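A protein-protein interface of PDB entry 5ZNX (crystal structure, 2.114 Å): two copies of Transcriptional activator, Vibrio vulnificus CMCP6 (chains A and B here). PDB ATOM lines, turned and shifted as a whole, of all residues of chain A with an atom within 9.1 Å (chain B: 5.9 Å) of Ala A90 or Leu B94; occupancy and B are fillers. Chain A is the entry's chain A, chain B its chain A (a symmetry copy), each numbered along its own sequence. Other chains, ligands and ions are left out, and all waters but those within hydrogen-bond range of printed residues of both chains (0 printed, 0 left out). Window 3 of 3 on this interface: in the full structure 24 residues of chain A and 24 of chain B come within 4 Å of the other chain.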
ATOM      1  N   ALA A  17      -6.319 -17.780  14.226  1.00  0.00           N
ATOM      2  CA  ALA A  17      -7.468 -18.672  14.125  1.00  0.00           C
ATOM      3  C   ALA A  17      -7.384 -19.538  12.874  1.00  0.00           C
ATOM      4  O   ALA A  17      -7.734 -20.725  12.914  1.00  0.00           O
ATOM      5  CB  ALA A  17      -8.764 -17.863  14.135  1.00  0.00           C
ATOM      6  N   LEU A  20      -5.281 -22.630  13.282  1.00  0.00           N
ATOM      7  CA  LEU A  20      -6.005 -23.689  13.973  1.00  0.00           C
ATOM      8  C   LEU A  20      -7.049 -24.327  13.064  1.00  0.00           C
ATOM      9  O   LEU A  20      -7.203 -25.555  13.055  1.00  0.00           O
ATOM     10  CB  LEU A  20      -6.651 -23.120  15.238  1.00  0.00           C
ATOM     11  CG  LEU A  20      -7.760 -23.895  15.948  1.00  0.00           C
ATOM     12  CD1 LEU A  20      -7.243 -25.225  16.457  1.00  0.00           C
ATOM     13  CD2 LEU A  20      -8.336 -23.067  17.091  1.00  0.00           C
ATOM     14  N   MET A  24      -7.408 -28.345  11.488  1.00  0.00           N
ATOM     15  CA  MET A  24      -8.573 -29.200  11.672  1.00  0.00           C
ATOM     16  C   MET A  24      -9.299 -29.511  10.371  1.00  0.00           C
ATOM     17  O   MET A  24     -10.089 -30.459  10.336  1.00  0.00           O
ATOM     18  CB  MET A  24      -9.579 -28.551  12.631  1.00  0.00           C
ATOM     19  CG  MET A  24      -9.009 -28.098  13.965  1.00  0.00           C
ATOM     20  SD  MET A  24     -10.191 -27.053  14.859  1.00  0.00           S
ATOM     21  CE  MET A  24     -11.479 -28.233  15.192  1.00  0.00           C
ATOM     22  N   HIS A  37     -10.828 -35.923  22.522  1.00  0.00           N
ATOM     23  CA  HIS A  37     -11.733 -35.092  23.307  1.00  0.00           C
ATOM     24  C   HIS A  37     -11.918 -35.727  24.679  1.00  0.00           C
ATOM     25  O   HIS A  37     -12.494 -36.814  24.791  1.00  0.00           O
ATOM     26  CB  HIS A  37     -13.067 -34.942  22.584  1.00  0.00           C
ATOM     27  CG  HIS A  37     -14.112 -34.245  23.392  1.00  0.00           C
ATOM     28  ND1 HIS A  37     -13.968 -32.950  23.837  1.00  0.00           N
ATOM     29  CD2 HIS A  37     -15.320 -34.666  23.840  1.00  0.00           C
ATOM     30  CE1 HIS A  37     -15.043 -32.599  24.520  1.00  0.00           C
ATOM     31  NE2 HIS A  37     -15.878 -33.621  24.535  1.00  0.00           N
ATOM     32  N   ASN A  38     -11.417 -35.056  25.721  1.00  0.00           N
ATOM     33  CA  ASN A  38     -11.497 -35.546  27.103  1.00  0.00           C
ATOM     34  C   ASN A  38     -10.906 -36.947  27.223  1.00  0.00           C
ATOM     35  O   ASN A  38     -11.420 -37.796  27.954  1.00  0.00           O
ATOM     36  CB  ASN A  38     -12.935 -35.532  27.624  1.00  0.00           C
ATOM     37  CG  ASN A  38     -13.512 -34.140  27.699  1.00  0.00           C
ATOM     38  OD1 ASN A  38     -12.788 -33.163  27.888  1.00  0.00           O
ATOM     39  ND2 ASN A  38     -14.826 -34.041  27.551  1.00  0.00           N
ATOM     40  N   LEU A  83      -5.178 -33.187  23.692  1.00  0.00           N
ATOM     41  CA  LEU A  83      -5.424 -31.841  23.182  1.00  0.00           C
ATOM     42  C   LEU A  83      -4.662 -30.857  24.057  1.00  0.00           C
ATOM     43  O   LEU A  83      -4.599 -31.017  25.280  1.00  0.00           O
ATOM     44  CB  LEU A  83      -6.919 -31.521  23.191  1.00  0.00           C
ATOM     45  CG  LEU A  83      -7.843 -32.404  22.347  1.00  0.00           C
ATOM     46  CD1 LEU A  83      -9.273 -31.867  22.385  1.00  0.00           C
ATOM     47  CD2 LEU A  83      -7.343 -32.497  20.922  1.00  0.00           C
ATOM     48  N   LYS A  84      -4.072 -29.838  23.429  1.00  0.00           N
ATOM     49  CA  LYS A  84      -3.249 -28.874  24.157  1.00  0.00           C
ATOM     50  C   LYS A  84      -3.894 -27.516  24.440  1.00  0.00           C
ATOM     51  O   LYS A  84      -4.062 -27.143  25.604  1.00  0.00           O
ATOM     52  CB  LYS A  84      -1.939 -28.657  23.382  1.00  0.00           C
ATOM     53  CG  LYS A  84      -0.997 -27.645  24.019  1.00  0.00           C
ATOM     54  CD  LYS A  84       0.334 -27.605  23.286  1.00  0.00           C
ATOM     55  CE  LYS A  84       1.325 -26.700  23.988  1.00  0.00           C
ATOM     56  NZ  LYS A  84       2.637 -26.705  23.293  1.00  0.00           N
ATOM     57  N   SER A  85      -4.231 -26.751  23.406  1.00  0.00           N
ATOM     58  CA  SER A  85      -4.750 -25.402  23.613  1.00  0.00           C
ATOM     59  C   SER A  85      -6.209 -25.375  24.051  1.00  0.00           C
ATOM     60  O   SER A  85      -7.017 -26.228  23.673  1.00  0.00           O
ATOM     61  CB  SER A  85      -4.601 -24.569  22.340  1.00  0.00           C
ATOM     62  OG  SER A  85      -5.649 -24.851  21.430  1.00  0.00           O
ATOM     63  N   GLU A  86      -6.541 -24.355  24.852  1.00  0.00           N
ATOM     64  CA  GLU A  86      -7.918 -24.194  25.307  1.00  0.00           C
ATOM     65  C   GLU A  86      -8.838 -23.900  24.134  1.00  0.00           C
ATOM     66  O   GLU A  86     -10.009 -24.296  24.149  1.00  0.00           O
ATOM     67  CB  GLU A  86      -8.014 -23.079  26.348  1.00  0.00           C
ATOM     68  CG  GLU A  86      -7.078 -23.251  27.533  1.00  0.00           C
ATOM     69  CD  GLU A  86      -7.011 -22.013  28.409  1.00  0.00           C
ATOM     70  OE1 GLU A  86      -7.729 -21.031  28.117  1.00  0.00           O
ATOM     71  OE2 GLU A  86      -6.237 -22.024  29.389  1.00  0.00           O
ATOM     72  N   GLU A  87      -8.320 -23.219  23.108  1.00  0.00           N
ATOM     73  CA  GLU A  87      -9.122 -22.916  21.929  1.00  0.00           C
ATOM     74  C   GLU A  87      -9.484 -24.189  21.173  1.00  0.00           C
ATOM     75  O   GLU A  87     -10.615 -24.330  20.693  1.00  0.00           O
ATOM     76  CB  GLU A  87      -8.374 -21.948  21.010  1.00  0.00           C
ATOM     77  CG  GLU A  87      -8.152 -20.562  21.594  1.00  0.00           C
ATOM     78  CD  GLU A  87      -7.048 -20.537  22.634  1.00  0.00           C
ATOM     79  OE1 GLU A  87      -6.288 -21.526  22.719  1.00  0.00           O
ATOM     80  OE2 GLU A  87      -6.944 -19.533  23.371  1.00  0.00           O
ATOM     81  N   VAL A  88      -8.541 -25.132  21.052  1.00  0.00           N
ATOM     82  CA  VAL A  88      -8.871 -26.363  20.341  1.00  0.00           C
ATOM     83  C   VAL A  88      -9.776 -27.236  21.201  1.00  0.00           C
ATOM     84  O   VAL A  88     -10.658 -27.926  20.675  1.00  0.00           O
ATOM     85  CB  VAL A  88      -7.601 -27.111  19.882  1.00  0.00           C
ATOM     86  CG1 VAL A  88      -6.994 -27.930  21.005  1.00  0.00           C
ATOM     87  CG2 VAL A  88      -7.932 -28.018  18.698  1.00  0.00           C
ATOM     88  N   LYS A  89      -9.600 -27.207  22.526  1.00  0.00           N
ATOM     89  CA  LYS A  89     -10.461 -28.002  23.396  1.00  0.00           C
ATOM     90  C   LYS A  89     -11.903 -27.526  23.288  1.00  0.00           C
ATOM     91  O   LYS A  89     -12.833 -28.340  23.241  1.00  0.00           O
ATOM     92  CB  LYS A  89      -9.973 -27.932  24.846  1.00  0.00           C
ATOM     93  CG  LYS A  89      -8.670 -28.690  25.109  1.00  0.00           C
ATOM     94  CD  LYS A  89      -8.282 -28.632  26.590  1.00  0.00           C
ATOM     95  CE  LYS A  89      -6.909 -29.248  26.842  1.00  0.00           C
ATOM     96  NZ  LYS A  89      -6.441 -29.051  28.248  1.00  0.00           N
ATOM     97  N   ALA A  90     -12.107 -26.206  23.233  1.00  0.00           N
ATOM     98  CA  ALA A  90     -13.460 -25.683  23.084  1.00  0.00           C
ATOM     99  C   ALA A  90     -14.002 -25.962  21.685  1.00  0.00           C
ATOM    100  O   ALA A  90     -15.204 -26.200  21.517  1.00  0.00           O
ATOM    101  CB  ALA A  90     -13.480 -24.182  23.384  1.00  0.00           C
ATOM    102  N   MET A  91     -13.129 -25.953  20.677  1.00  0.00           N
ATOM    103  CA  MET A  91     -13.556 -26.225  19.308  1.00  0.00           C
ATOM    104  C   MET A  91     -14.027 -27.667  19.152  1.00  0.00           C
ATOM    105  O   MET A  91     -15.083 -27.931  18.561  1.00  0.00           O
ATOM    106  CB  MET A  91     -12.402 -25.935  18.349  1.00  0.00           C
ATOM    107  CG  MET A  91     -12.434 -24.544  17.792  1.00  0.00           C
ATOM    108  SD  MET A  91     -13.985 -24.337  16.919  1.00  0.00           S
ATOM    109  CE  MET A  91     -14.279 -22.600  17.180  1.00  0.00           C
ATOM    110  N   ILE A  92     -13.249 -28.616  19.673  1.00  0.00           N
ATOM    111  CA  ILE A  92     -13.618 -30.022  19.563  1.00  0.00           C
ATOM    112  C   ILE A  92     -14.863 -30.315  20.390  1.00  0.00           C
ATOM    113  O   ILE A  92     -15.729 -31.097  19.978  1.00  0.00           O
ATOM    114  CB  ILE A  92     -12.426 -30.902  19.976  1.00  0.00           C
ATOM    115  CG1 ILE A  92     -11.262 -30.659  19.019  1.00  0.00           C
ATOM    116  CG2 ILE A  92     -12.817 -32.368  19.983  1.00  0.00           C
ATOM    117  CD1 ILE A  92     -11.609 -30.960  17.575  1.00  0.00           C
ATOM    118  N   LYS A  93     -14.979 -29.685  21.562  1.00  0.00           N
ATOM    119  CA  LYS A  93     -16.155 -29.897  22.399  1.00  0.00           C
ATOM    120  C   LYS A  93     -17.427 -29.507  21.656  1.00  0.00           C
ATOM    121  O   LYS A  93     -18.431 -30.226  21.701  1.00  0.00           O
ATOM    122  CB  LYS A  93     -16.016 -29.100  23.696  1.00  0.00           C
ATOM    123  CG  LYS A  93     -17.174 -29.266  24.669  1.00  0.00           C
ATOM    124  CD  LYS A  93     -16.927 -28.436  25.923  1.00  0.00           C
ATOM    125  CE  LYS A  93     -18.178 -28.320  26.777  1.00  0.00           C
ATOM    126  NZ  LYS A  93     -17.943 -27.456  27.970  1.00  0.00           N
ATOM    127  N   LEU A  94     -17.396 -28.375  20.947  1.00  0.00           N
ATOM    128  CA  LEU A  94     -18.569 -27.952  20.189  1.00  0.00           C
ATOM    129  C   LEU A  94     -18.809 -28.869  18.997  1.00  0.00           C
ATOM    130  O   LEU A  94     -19.952 -29.254  18.724  1.00  0.00           O
ATOM    131  CB  LEU A  94     -18.399 -26.505  19.729  1.00  0.00           C
ATOM    132  CG  LEU A  94     -19.463 -25.967  18.774  1.00  0.00           C
ATOM    133  CD1 LEU A  94     -20.853 -26.031  19.408  1.00  0.00           C
ATOM    134  CD2 LEU A  94     -19.112 -24.544  18.362  1.00  0.00           C
ATOM    135  N   LEU A  95     -17.747 -29.240  18.278  1.00  0.00           N
ATOM    136  CA  LEU A  95     -17.918 -30.126  17.130  1.00  0.00           C
ATOM    137  C   LEU A  95     -18.434 -31.486  17.570  1.00  0.00           C
ATOM    138  O   LEU A  95     -19.256 -32.102  16.878  1.00  0.00           O
ATOM    139  CB  LEU A  95     -16.599 -30.282  16.373  1.00  0.00           C
ATOM    140  CG  LEU A  95     -16.274 -29.153  15.397  1.00  0.00           C
ATOM    141  CD1 LEU A  95     -14.825 -29.200  14.954  1.00  0.00           C
ATOM    142  CD2 LEU A  95     -17.207 -29.188  14.194  1.00  0.00           C
ATOM    143  N   HIS A  96     -17.967 -31.966  18.725  1.00  0.00           N
ATOM    144  CA  HIS A  96     -18.406 -33.260  19.231  1.00  0.00           C
ATOM    145  C   HIS A  96     -19.921 -33.305  19.398  1.00  0.00           C
ATOM    146  O   HIS A  96     -20.562 -34.301  19.043  1.00  0.00           O
ATOM    147  CB  HIS A  96     -17.713 -33.557  20.562  1.00  0.00           C
ATOM    148  CG  HIS A  96     -17.555 -35.017  20.846  1.00  0.00           C
ATOM    149  ND1 HIS A  96     -18.402 -35.707  21.683  1.00  0.00           N
ATOM    150  CD2 HIS A  96     -16.646 -35.917  20.400  1.00  0.00           C
ATOM    151  CE1 HIS A  96     -18.024 -36.972  21.742  1.00  0.00           C
ATOM    152  NE2 HIS A  96     -16.963 -37.125  20.972  1.00  0.00           N
ATOM    153  N   SER A  97     -20.513 -32.236  19.932  1.00  0.00           N
ATOM    154  CA  SER A  97     -21.957 -32.212  20.123  1.00  0.00           C
ATOM    155  C   SER A  97     -22.719 -32.013  18.822  1.00  0.00           C
ATOM    156  O   SER A  97     -23.899 -32.370  18.751  1.00  0.00           O
ATOM    157  CB  SER A  97     -22.345 -31.116  21.119  1.00  0.00           C
ATOM    158  OG  SER A  97     -21.945 -29.836  20.666  1.00  0.00           O
ATOM    159  N   LEU A  98     -22.077 -31.461  17.795  1.00  0.00           N
ATOM    160  CA  LEU A  98     -22.748 -31.232  16.522  1.00  0.00           C
ATOM    161  C   LEU A  98     -22.654 -32.412  15.566  1.00  0.00           C
ATOM    162  O   LEU A  98     -23.545 -32.582  14.724  1.00  0.00           O
ATOM    163  CB  LEU A  98     -22.166 -29.992  15.833  1.00  0.00           C
ATOM    164  CG  LEU A  98     -22.329 -28.631  16.510  1.00  0.00           C
ATOM    165  CD1 LEU A  98     -21.347 -27.627  15.920  1.00  0.00           C
ATOM    166  CD2 LEU A  98     -23.751 -28.125  16.365  1.00  0.00           C
ATOM    167  N   LYS B  89     -23.261 -20.903  12.752  1.00  0.00           N
ATOM    168  CA  LYS B  89     -23.605 -19.869  13.723  1.00  0.00           C
ATOM    169  C   LYS B  89     -22.978 -20.183  15.074  1.00  0.00           C
ATOM    170  O   LYS B  89     -22.462 -19.287  15.751  1.00  0.00           O
ATOM    171  CB  LYS B  89     -25.125 -19.733  13.848  1.00  0.00           C
ATOM    172  CG  LYS B  89     -25.804 -19.099  12.631  1.00  0.00           C
ATOM    173  CD  LYS B  89     -27.310 -18.936  12.857  1.00  0.00           C
ATOM    174  CE  LYS B  89     -28.024 -18.451  11.598  1.00  0.00           C
ATOM    175  NZ  LYS B  89     -29.511 -18.445  11.747  1.00  0.00           N
ATOM    176  N   ALA B  90     -23.001 -21.458  15.475  1.00  0.00           N
ATOM    177  CA  ALA B  90     -22.378 -21.836  16.738  1.00  0.00           C
ATOM    178  C   ALA B  90     -20.857 -21.751  16.644  1.00  0.00           C
ATOM    179  O   ALA B  90     -20.189 -21.408  17.626  1.00  0.00           O
ATOM    180  CB  ALA B  90     -22.820 -23.245  17.141  1.00  0.00           C
ATOM    181  N   MET B  91     -20.300 -22.045  15.468  1.00  0.00           N
ATOM    182  CA  MET B  91     -18.854 -21.974  15.283  1.00  0.00           C
ATOM    183  C   MET B  91     -18.351 -20.539  15.391  1.00  0.00           C
ATOM    184  O   MET B  91     -17.355 -20.263  16.074  1.00  0.00           O
ATOM    185  CB  MET B  91     -18.487 -22.566  13.922  1.00  0.00           C
ATOM    186  CG  MET B  91     -18.134 -24.021  13.989  1.00  0.00           C
ATOM    187  SD  MET B  91     -16.737 -24.198  15.097  1.00  0.00           S
ATOM    188  CE  MET B  91     -17.059 -25.812  15.776  1.00  0.00           C
ATOM    189  N   ILE B  92     -19.027 -19.610  14.714  1.00  0.00           N
ATOM    190  CA  ILE B  92     -18.612 -18.213  14.753  1.00  0.00           C
ATOM    191  C   ILE B  92     -18.821 -17.632  16.145  1.00  0.00           C
ATOM    192  O   ILE B  92     -18.004 -16.840  16.632  1.00  0.00           O
ATOM    193  CB  ILE B  92     -19.367 -17.420  13.673  1.00  0.00           C
ATOM    194  CG1 ILE B  92     -19.000 -17.967  12.295  1.00  0.00           C
ATOM    195  CG2 ILE B  92     -19.041 -15.941  13.765  1.00  0.00           C
ATOM    196  CD1 ILE B  92     -17.516 -17.892  12.003  1.00  0.00           C
ATOM    197  N   LYS B  93     -19.910 -18.023  16.812  1.00  0.00           N
ATOM    198  CA  LYS B  93     -20.166 -17.526  18.160  1.00  0.00           C
ATOM    199  C   LYS B  93     -19.022 -17.891  19.098  1.00  0.00           C
ATOM    200  O   LYS B  93     -18.570 -17.061  19.896  1.00  0.00           O
ATOM    201  CB  LYS B  93     -21.492 -18.087  18.674  1.00  0.00           C
ATOM    202  CG  LYS B  93     -21.884 -17.613  20.065  1.00  0.00           C
ATOM    203  CD  LYS B  93     -23.219 -18.227  20.471  1.00  0.00           C
ATOM    204  CE  LYS B  93     -23.499 -18.039  21.952  1.00  0.00           C
ATOM    205  NZ  LYS B  93     -24.777 -18.696  22.351  1.00  0.00           N
ATOM    206  N   LEU B  94     -18.526 -19.127  19.003  1.00  0.00           N
ATOM    207  CA  LEU B  94     -17.413 -19.538  19.852  1.00  0.00           C
ATOM    208  C   LEU B  94     -16.127 -18.829  19.449  1.00  0.00           C
ATOM    209  O   LEU B  94     -15.370 -18.367  20.310  1.00  0.00           O
ATOM    210  CB  LEU B  94     -17.236 -21.054  19.783  1.00  0.00           C
ATOM    211  CG  LEU B  94     -16.001 -21.626  20.478  1.00  0.00           C
ATOM    212  CD1 LEU B  94     -16.004 -21.286  21.968  1.00  0.00           C
ATOM    213  CD2 LEU B  94     -15.939 -23.131  20.258  1.00  0.00           C
ATOM    214  N   LEU B  95     -15.863 -18.721  18.144  1.00  0.00           N
ATOM    215  CA  LEU B  95     -14.649 -18.042  17.700  1.00  0.00           C
ATOM    216  C   LEU B  95     -14.677 -16.574  18.091  1.00  0.00           C
ATOM    217  O   LEU B  95     -13.644 -16.000  18.461  1.00  0.00           O
ATOM    218  CB  LEU B  95     -14.480 -18.182  16.187  1.00  0.00           C
ATOM    219  CG  LEU B  95     -13.860 -19.499  15.722  1.00  0.00           C
ATOM    220  CD1 LEU B  95     -14.042 -19.703  14.232  1.00  0.00           C
ATOM    221  CD2 LEU B  95     -12.387 -19.570  16.101  1.00  0.00           C
ATOM    222  N   HIS B  96     -15.857 -15.953  18.024  1.00  0.00           N
ATOM    223  CA  HIS B  96     -15.985 -14.546  18.383  1.00  0.00           C
ATOM    224  C   HIS B  96     -15.516 -14.293  19.811  1.00  0.00           C
ATOM    225  O   HIS B  96     -14.816 -13.309  20.076  1.00  0.00           O
ATOM    226  CB  HIS B  96     -17.437 -14.098  18.210  1.00  0.00           C
ATOM    227  CG  HIS B  96     -17.587 -12.640  17.913  1.00  0.00           C
ATOM    228  ND1 HIS B  96     -17.919 -11.716  18.877  1.00  0.00           N
ATOM    229  CD2 HIS B  96     -17.445 -11.948  16.757  1.00  0.00           C
ATOM    230  CE1 HIS B  96     -17.978 -10.514  18.329  1.00  0.00           C
ATOM    231  NE2 HIS B  96     -17.693 -10.628  17.045  1.00  0.00           N
ATOM    232  N   SER B  97     -15.885 -15.172  20.744  1.00  0.00           N
ATOM    233  CA  SER B  97     -15.475 -14.990  22.130  1.00  0.00           C
ATOM    234  C   SER B  97     -14.010 -15.329  22.359  1.00  0.00           C
ATOM    235  O   SER B  97     -13.424 -14.854  23.336  1.00  0.00           O
ATOM    236  CB  SER B  97     -16.348 -15.836  23.060  1.00  0.00           C
ATOM    237  OG  SER B  97     -16.252 -17.214  22.755  1.00  0.00           O
ATOM    238  N   LEU B  98     -13.405 -16.129  21.483  1.00  0.00           N
ATOM    239  CA  LEU B  98     -12.006 -16.502  21.646  1.00  0.00           C
ATOM    240  C   LEU B  98     -11.038 -15.533  20.982  1.00  0.00           C
ATOM    241  O   LEU B  98      -9.894 -15.413  21.437  1.00  0.00           O
ATOM    242  CB  LEU B  98     -11.764 -17.906  21.077  1.00  0.00           C
ATOM    243  CG  LEU B  98     -12.472 -19.094  21.729  1.00  0.00           C
ATOM    244  CD1 LEU B  98     -12.455 -20.296  20.794  1.00  0.00           C
ATOM    245  CD2 LEU B  98     -11.823 -19.446  23.053  1.00  0.00           C
ATOM    246  N   TYR B  99     -11.452 -14.841  19.918  1.00  0.00           N
ATOM    247  CA  TYR B  99     -10.539 -13.931  19.235  1.00  0.00           C
ATOM    248  C   TYR B  99     -11.094 -12.526  19.012  1.00  0.00           C
ATOM    249  O   TYR B  99     -10.330 -11.555  19.007  1.00  0.00           O
ATOM    250  CB  TYR B  99     -10.128 -14.530  17.885  1.00  0.00           C
ATOM    251  CG  TYR B  99      -9.487 -15.901  17.979  1.00  0.00           C
ATOM    252  CD1 TYR B  99      -8.115 -16.037  18.167  1.00  0.00           C
ATOM    253  CD2 TYR B  99     -10.250 -17.056  17.875  1.00  0.00           C
ATOM    254  CE1 TYR B  99      -7.523 -17.287  18.251  1.00  0.00           C
ATOM    255  CE2 TYR B  99      -9.666 -18.312  17.957  1.00  0.00           C
ATOM    256  CZ  TYR B  99      -8.303 -18.420  18.146  1.00  0.00           C
ATOM    257  OH  TYR B  99      -7.720 -19.667  18.229  1.00  0.00           O
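The side-chain sulfur (SD) of Met B91 lies close to the side-chain sulfur (SD) of Met A91, 3.3 Å away.
Ala A90 touches Leu B94, and with the chains exchanged Leu A94 touches Ala B90.
Met B91 touches its own counterpart, Met A91.
Met A91 touches Leu B95, and with the chains exchanged Leu A95 touches Met B91.
Leu A94 touches its own counterpart, Leu B94.
10 positions are printed for both chains.
Of the 11 pairs that touch across the chains among the printed residues, 8 have their exchanged pair printed and touching as well.
The backbone carbonyl oxygen of Leu A94 lies within hydrogen-bond range of the side-chain hydroxyl of Ser A97.
OG of Ser B97 lies within hydrogen-bond range of O of Leu B94, at 2.8 Å.
Tyr B99 touches Ala A17.
Leu A20 touches Tyr B99.
Glu A87 touches Tyr B99.
O of Ala A90 touches CD2 of Leu B94, 3.4 Å away.
CD2 of Leu B94 touches CE of Met A91 (3.5 Å).
Met A91 touches Leu B95 (CE to CG, 3.5 Å).
Ala B90 touches Leu A94 (O to CD2, 3.4 Å).
Met B91 touches Leu A94 (CE to CD2, 3.5 Å).
Leu A94 touches Leu B94.
Leu A95 touches Met B91 (CG to CE, 3.5 Å).
Of the printed residues of chain B, Ala A17 touches Tyr B99 (3.95 Å).
Of the printed residues of chain B, Leu A20 touches Tyr B99 (3.6 Å).
Ala A90 touches just one residue of chain B: Leu B94 (3.4 Å).
Printed residues of chain B within 4 Å of Leu A94: Ala B90 (3.4 Å), Met B91 (3.5 Å) and Leu B94 (3.96 Å).
Leu B94 touches just these residues of chain A: Ala A90 (3.4 Å), Met A91 (3.5 Å) and Leu A94 (3.96 Å).
Of the printed residues of chain A, Leu B95 touches Met A91 (3.5 Å).
No residue of chain A comes within 4 Å of Ser B97.
Of the printed residues of chain A, Tyr B99 touches Ala A17 (3.95 Å), Leu A20 (3.6 Å) and Glu A87 (3.5 Å).
The nearest residue of chain B that does not touch Ala A90 is Leu B98 (4.8 Å).
The nearest printed residue of chain B that does not touch Met A91 is Leu B98 (4.7 Å).
Hydrophobic or aromatic side chains of chain B within 4 Å of the printed part of chain A: Met B91, Leu B94, Leu B95 and Tyr B99.
Of the 21 printed residues of chain A, 7 touch a printed residue of chain B.
Among the printed residues, 11 pairs touch across the chains.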
